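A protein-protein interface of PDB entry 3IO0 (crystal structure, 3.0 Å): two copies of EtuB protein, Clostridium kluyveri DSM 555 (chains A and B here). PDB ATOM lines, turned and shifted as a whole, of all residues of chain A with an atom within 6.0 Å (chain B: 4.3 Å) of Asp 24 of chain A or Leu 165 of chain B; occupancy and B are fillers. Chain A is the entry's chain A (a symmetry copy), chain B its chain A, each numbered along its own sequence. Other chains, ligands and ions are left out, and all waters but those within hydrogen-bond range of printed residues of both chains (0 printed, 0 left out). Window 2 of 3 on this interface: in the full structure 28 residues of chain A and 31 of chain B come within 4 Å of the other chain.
The side-chain carboxylate of Asp 162 of chain B lies within hydrogen-bond range of the backbone NH of Asp 24 of chain A, at 3.0 Å. The backbone carbonyl oxygen of Asn 22 of chain A sits at hydrogen-bond distance from the side-chain amino group of Lys 166 of chain B, at 2.6 Å.
OD2 of Asp 162 of chain B lies within salt-bridge range of NZ of Lys 166 of chain B, 3.1 Å away. The backbone carbonyl oxygen of Val 23 of chain A is in hydrogen-bond range of a ring nitrogen (NE2) of His 28 of chain A. The side-chain carboxylate (OD2) of Asp 24 of chain A lies within hydrogen-bond range of the backbone NH (N) of Leu 26 of chain A (3.0 Å).
Among the printed residues, pairs that only touch across the chains: Asp 24 of chain A with Leu 165 of chain B (3.5 Å), Ile 20 of chain A with Asp 162 of chain B (3.6 Å), Asp 24 of chain A with Lys 166 of chain B (3.6 Å), Leu 26 of chain A with Leu 172 of chain B (3.7 Å), Leu 27 of chain A with Leu 165 of chain B (3.7 Å), Val 23 of chain A with Asp 162 of chain B (3.7 Å), Leu 26 of chain A with Leu 165 of chain B (3.9 Å) and Leu 27 of chain A with Asp 162 of chain B (3.98 Å).
Of the printed residues of chain B, Ile 20 of chain A touches Asp 162. Of chain B, only Asp 162, Leu 165 and Lys 166 come within 4 Å of Asp 24 of chain A. Printed residues of chain B within 4 Å of Leu 27 of chain A: Asp 162 (3.98 Å) and Leu 165 (3.7 Å). Leu 165 of chain B touches three residues of chain A. The nearest printed residue of chain B that does not touch Asp 24 of chain A is Thr 167 of chain B (6.0 Å).
Hydrophobic or aromatic side chains of chain B that line the printed part of chain A: Leu 165 and Leu 172.
No position is printed for both chains.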
ATOM      1  N   ILE A  20      -3.688 -12.026 -24.535  1.00  0.00           N
ATOM      2  CA  ILE A  20      -2.584 -11.268 -23.953  1.00  0.00           C
ATOM      3  C   ILE A  20      -2.894 -10.970 -22.495  1.00  0.00           C
ATOM      4  O   ILE A  20      -3.943 -10.418 -22.172  1.00  0.00           O
ATOM      5  CB  ILE A  20      -2.236  -9.980 -24.732  1.00  0.00           C
ATOM      6  CG1 ILE A  20      -1.672 -10.337 -26.110  1.00  0.00           C
ATOM      7  CG2 ILE A  20      -1.240  -9.105 -23.934  1.00  0.00           C
ATOM      8  CD1 ILE A  20      -1.336  -9.142 -27.002  1.00  0.00           C
ATOM      9  N   ASN A  22      -1.271  -9.047 -20.010  1.00  0.00           N
ATOM     10  CA  ASN A  22      -1.191  -7.705 -19.473  1.00  0.00           C
ATOM     11  C   ASN A  22      -0.797  -6.688 -20.516  1.00  0.00           C
ATOM     12  O   ASN A  22       0.373  -6.330 -20.620  1.00  0.00           O
ATOM     13  CB  ASN A  22      -0.196  -7.682 -18.321  1.00  0.00           C
ATOM     14  CG  ASN A  22      -0.872  -7.547 -16.980  1.00  0.00           C
ATOM     15  OD1 ASN A  22      -0.938  -8.500 -16.198  1.00  0.00           O
ATOM     16  ND2 ASN A  22      -1.385  -6.356 -16.705  1.00  0.00           N
ATOM     17  N   VAL A  23      -1.773  -6.208 -21.281  1.00  0.00           N
ATOM     18  CA  VAL A  23      -1.490  -5.388 -22.459  1.00  0.00           C
ATOM     19  C   VAL A  23      -0.705  -4.149 -22.071  1.00  0.00           C
ATOM     20  O   VAL A  23      -1.041  -3.485 -21.095  1.00  0.00           O
ATOM     21  CB  VAL A  23      -2.787  -5.003 -23.210  1.00  0.00           C
ATOM     22  CG1 VAL A  23      -2.484  -4.138 -24.438  1.00  0.00           C
ATOM     23  CG2 VAL A  23      -3.550  -6.249 -23.615  1.00  0.00           C
ATOM     24  N   ASP A  24       0.352  -3.860 -22.824  1.00  0.00           N
ATOM     25  CA  ASP A  24       1.156  -2.673 -22.570  1.00  0.00           C
ATOM     26  C   ASP A  24       0.279  -1.440 -22.516  1.00  0.00           C
ATOM     27  O   ASP A  24      -0.593  -1.263 -23.362  1.00  0.00           O
ATOM     28  CB  ASP A  24       2.244  -2.497 -23.623  1.00  0.00           C
ATOM     29  CG  ASP A  24       3.290  -1.477 -23.201  1.00  0.00           C
ATOM     30  OD1 ASP A  24       4.386  -1.906 -22.754  1.00  0.00           O
ATOM     31  OD2 ASP A  24       3.003  -0.253 -23.283  1.00  0.00           O
ATOM     32  N   SER A  25       0.518  -0.587 -21.528  1.00  0.00           N
ATOM     33  CA  SER A  25      -0.367   0.547 -21.268  1.00  0.00           C
ATOM     34  C   SER A  25      -0.440   1.571 -22.416  1.00  0.00           C
ATOM     35  O   SER A  25      -1.415   2.320 -22.538  1.00  0.00           O
ATOM     36  CB  SER A  25       0.015   1.221 -19.955  1.00  0.00           C
ATOM     37  OG  SER A  25       1.184   1.990 -20.132  1.00  0.00           O
ATOM     38  N   LEU A  26       0.586   1.590 -23.259  1.00  0.00           N
ATOM     39  CA  LEU A  26       0.577   2.441 -24.448  1.00  0.00           C
ATOM     40  C   LEU A  26      -0.532   2.069 -25.441  1.00  0.00           C
ATOM     41  O   LEU A  26      -0.938   2.892 -26.261  1.00  0.00           O
ATOM     42  CB  LEU A  26       1.940   2.411 -25.143  1.00  0.00           C
ATOM     43  CG  LEU A  26       3.092   3.123 -24.439  1.00  0.00           C
ATOM     44  CD1 LEU A  26       4.414   2.670 -25.024  1.00  0.00           C
ATOM     45  CD2 LEU A  26       2.940   4.627 -24.554  1.00  0.00           C
ATOM     46  N   LEU A  27      -1.022   0.838 -25.361  1.00  0.00           N
ATOM     47  CA  LEU A  27      -2.083   0.373 -26.244  1.00  0.00           C
ATOM     48  C   LEU A  27      -3.475   0.501 -25.627  1.00  0.00           C
ATOM     49  O   LEU A  27      -4.485   0.241 -26.297  1.00  0.00           O
ATOM     50  CB  LEU A  27      -1.840  -1.084 -26.620  1.00  0.00           C
ATOM     51  CG  LEU A  27      -0.678  -1.398 -27.550  1.00  0.00           C
ATOM     52  CD1 LEU A  27      -0.448  -2.893 -27.592  1.00  0.00           C
ATOM     53  CD2 LEU A  27      -0.937  -0.854 -28.941  1.00  0.00           C
ATOM     54  N   HIS A  28      -3.522   0.883 -24.348  1.00  0.00           N
ATOM     55  CA  HIS A  28      -4.771   0.936 -23.590  1.00  0.00           C
ATOM     56  C   HIS A  28      -5.736   1.933 -24.188  1.00  0.00           C
ATOM     57  O   HIS A  28      -6.902   1.631 -24.356  1.00  0.00           O
ATOM     58  CB  HIS A  28      -4.500   1.293 -22.134  1.00  0.00           C
ATOM     59  CG  HIS A  28      -3.910   0.178 -21.335  1.00  0.00           C
ATOM     60  ND1 HIS A  28      -3.875   0.193 -19.958  1.00  0.00           N
ATOM     61  CD2 HIS A  28      -3.340  -0.989 -21.713  1.00  0.00           C
ATOM     62  CE1 HIS A  28      -3.300  -0.912 -19.523  1.00  0.00           C
ATOM     63  NE2 HIS A  28      -2.968  -1.647 -20.568  1.00  0.00           N
ATOM     64  N   ALA B 161       2.935  -6.271 -31.928  1.00  0.00           N
ATOM     65  CA  ALA B 161       2.873  -4.893 -31.446  1.00  0.00           C
ATOM     66  C   ALA B 161       3.113  -4.784 -29.943  1.00  0.00           C
ATOM     67  O   ALA B 161       3.921  -3.973 -29.484  1.00  0.00           O
ATOM     68  CB  ALA B 161       1.542  -4.284 -31.807  1.00  0.00           C
ATOM     69  N   ASP B 162       2.400  -5.607 -29.189  1.00  0.00           N
ATOM     70  CA  ASP B 162       2.484  -5.584 -27.744  1.00  0.00           C
ATOM     71  C   ASP B 162       3.881  -5.984 -27.246  1.00  0.00           C
ATOM     72  O   ASP B 162       4.451  -5.277 -26.404  1.00  0.00           O
ATOM     73  CB  ASP B 162       1.372  -6.448 -27.137  1.00  0.00           C
ATOM     74  CG  ASP B 162       1.564  -6.708 -25.653  1.00  0.00           C
ATOM     75  OD1 ASP B 162       1.372  -5.757 -24.850  1.00  0.00           O
ATOM     76  OD2 ASP B 162       1.893  -7.872 -25.300  1.00  0.00           O
ATOM     77  N   THR B 163       4.458  -7.074 -27.768  1.00  0.00           N
ATOM     78  CA  THR B 163       5.772  -7.487 -27.244  1.00  0.00           C
ATOM     79  C   THR B 163       6.880  -6.506 -27.632  1.00  0.00           C
ATOM     80  O   THR B 163       7.873  -6.371 -26.917  1.00  0.00           O
ATOM     81  CB  THR B 163       6.199  -8.973 -27.540  1.00  0.00           C
ATOM     82  OG1 THR B 163       6.787  -9.074 -28.835  1.00  0.00           O
ATOM     83  CG2 THR B 163       5.036  -9.980 -27.379  1.00  0.00           C
ATOM     84  N   ALA B 164       6.695  -5.805 -28.747  1.00  0.00           N
ATOM     85  CA  ALA B 164       7.635  -4.769 -29.137  1.00  0.00           C
ATOM     86  C   ALA B 164       7.702  -3.699 -28.057  1.00  0.00           C
ATOM     87  O   ALA B 164       8.787  -3.293 -27.654  1.00  0.00           O
ATOM     88  CB  ALA B 164       7.245  -4.166 -30.452  1.00  0.00           C
ATOM     89  N   LEU B 165       6.541  -3.270 -27.570  1.00  0.00           N
ATOM     90  CA  LEU B 165       6.452  -2.152 -26.637  1.00  0.00           C
ATOM     91  C   LEU B 165       6.901  -2.539 -25.233  1.00  0.00           C
ATOM     92  O   LEU B 165       7.451  -1.714 -24.480  1.00  0.00           O
ATOM     93  CB  LEU B 165       5.019  -1.630 -26.598  1.00  0.00           C
ATOM     94  CG  LEU B 165       4.463  -0.993 -27.871  1.00  0.00           C
ATOM     95  CD1 LEU B 165       2.954  -0.909 -27.793  1.00  0.00           C
ATOM     96  CD2 LEU B 165       5.053   0.386 -28.069  1.00  0.00           C
ATOM     97  N   LYS B 166       6.643  -3.801 -24.893  1.00  0.00           N
ATOM     98  CA  LYS B 166       7.063  -4.388 -23.623  1.00  0.00           C
ATOM     99  C   LYS B 166       8.587  -4.509 -23.558  1.00  0.00           C
ATOM    100  O   LYS B 166       9.183  -4.235 -22.527  1.00  0.00           O
ATOM    101  CB  LYS B 166       6.421  -5.766 -23.439  1.00  0.00           C
ATOM    102  CG  LYS B 166       4.975  -5.769 -22.923  1.00  0.00           C
ATOM    103  CD  LYS B 166       4.315  -7.094 -23.325  1.00  0.00           C
ATOM    104  CE  LYS B 166       3.498  -7.760 -22.208  1.00  0.00           C
ATOM    105  NZ  LYS B 166       2.060  -7.450 -22.273  1.00  0.00           N
ATOM    106  N   THR B 167       9.195  -4.888 -24.682  1.00  0.00           N
ATOM    107  CA  THR B 167      10.617  -5.219 -24.775  1.00  0.00           C
ATOM    108  C   THR B 167      11.601  -4.107 -24.418  1.00  0.00           C
ATOM    109  O   THR B 167      12.653  -4.385 -23.841  1.00  0.00           O
ATOM    110  CB  THR B 167      10.949  -5.741 -26.182  1.00  0.00           C
ATOM    111  OG1 THR B 167      10.473  -7.080 -26.299  1.00  0.00           O
ATOM    112  CG2 THR B 167      12.451  -5.723 -26.458  1.00  0.00           C
ATOM    113  N   ALA B 168      11.291  -2.863 -24.766  1.00  0.00           N
ATOM    114  CA  ALA B 168      12.262  -1.790 -24.589  1.00  0.00           C
ATOM    115  C   ALA B 168      11.588  -0.448 -24.413  1.00  0.00           C
ATOM    116  O   ALA B 168      10.354  -0.349 -24.452  1.00  0.00           O
ATOM    117  CB  ALA B 168      13.233  -1.753 -25.765  1.00  0.00           C
ATOM    118  N   LEU B 172       5.474   5.043 -28.942  1.00  0.00           N
ATOM    119  CA  LEU B 172       4.466   4.527 -29.865  1.00  0.00           C
ATOM    120  C   LEU B 172       4.044   5.674 -30.754  1.00  0.00           C
ATOM    121  O   LEU B 172       3.445   6.629 -30.284  1.00  0.00           O
ATOM    122  CB  LEU B 172       3.242   4.022 -29.108  1.00  0.00           C
ATOM    123  CG  LEU B 172       2.313   2.951 -29.699  1.00  0.00           C
ATOM    124  CD1 LEU B 172       0.854   3.323 -29.417  1.00  0.00           C
ATOM    125  CD2 LEU B 172       2.511   2.712 -31.184  1.00  0.00           C
ATOM    126  N   ILE B 193       7.161   2.844 -34.384  1.00  0.00           N
ATOM    127  CA  ILE B 193       7.950   3.023 -33.168  1.00  0.00           C
ATOM    128  C   ILE B 193       9.175   3.918 -33.371  1.00  0.00           C
ATOM    129  O   ILE B 193       9.817   3.863 -34.425  1.00  0.00           O
ATOM    130  CB  ILE B 193       8.216   1.623 -32.541  1.00  0.00           C
ATOM    131  CG1 ILE B 193       7.388   1.515 -31.274  1.00  0.00           C
ATOM    132  CG2 ILE B 193       9.699   1.284 -32.321  1.00  0.00           C
ATOM    133  CD1 ILE B 193       6.972   0.112 -30.952  1.00  0.00           C
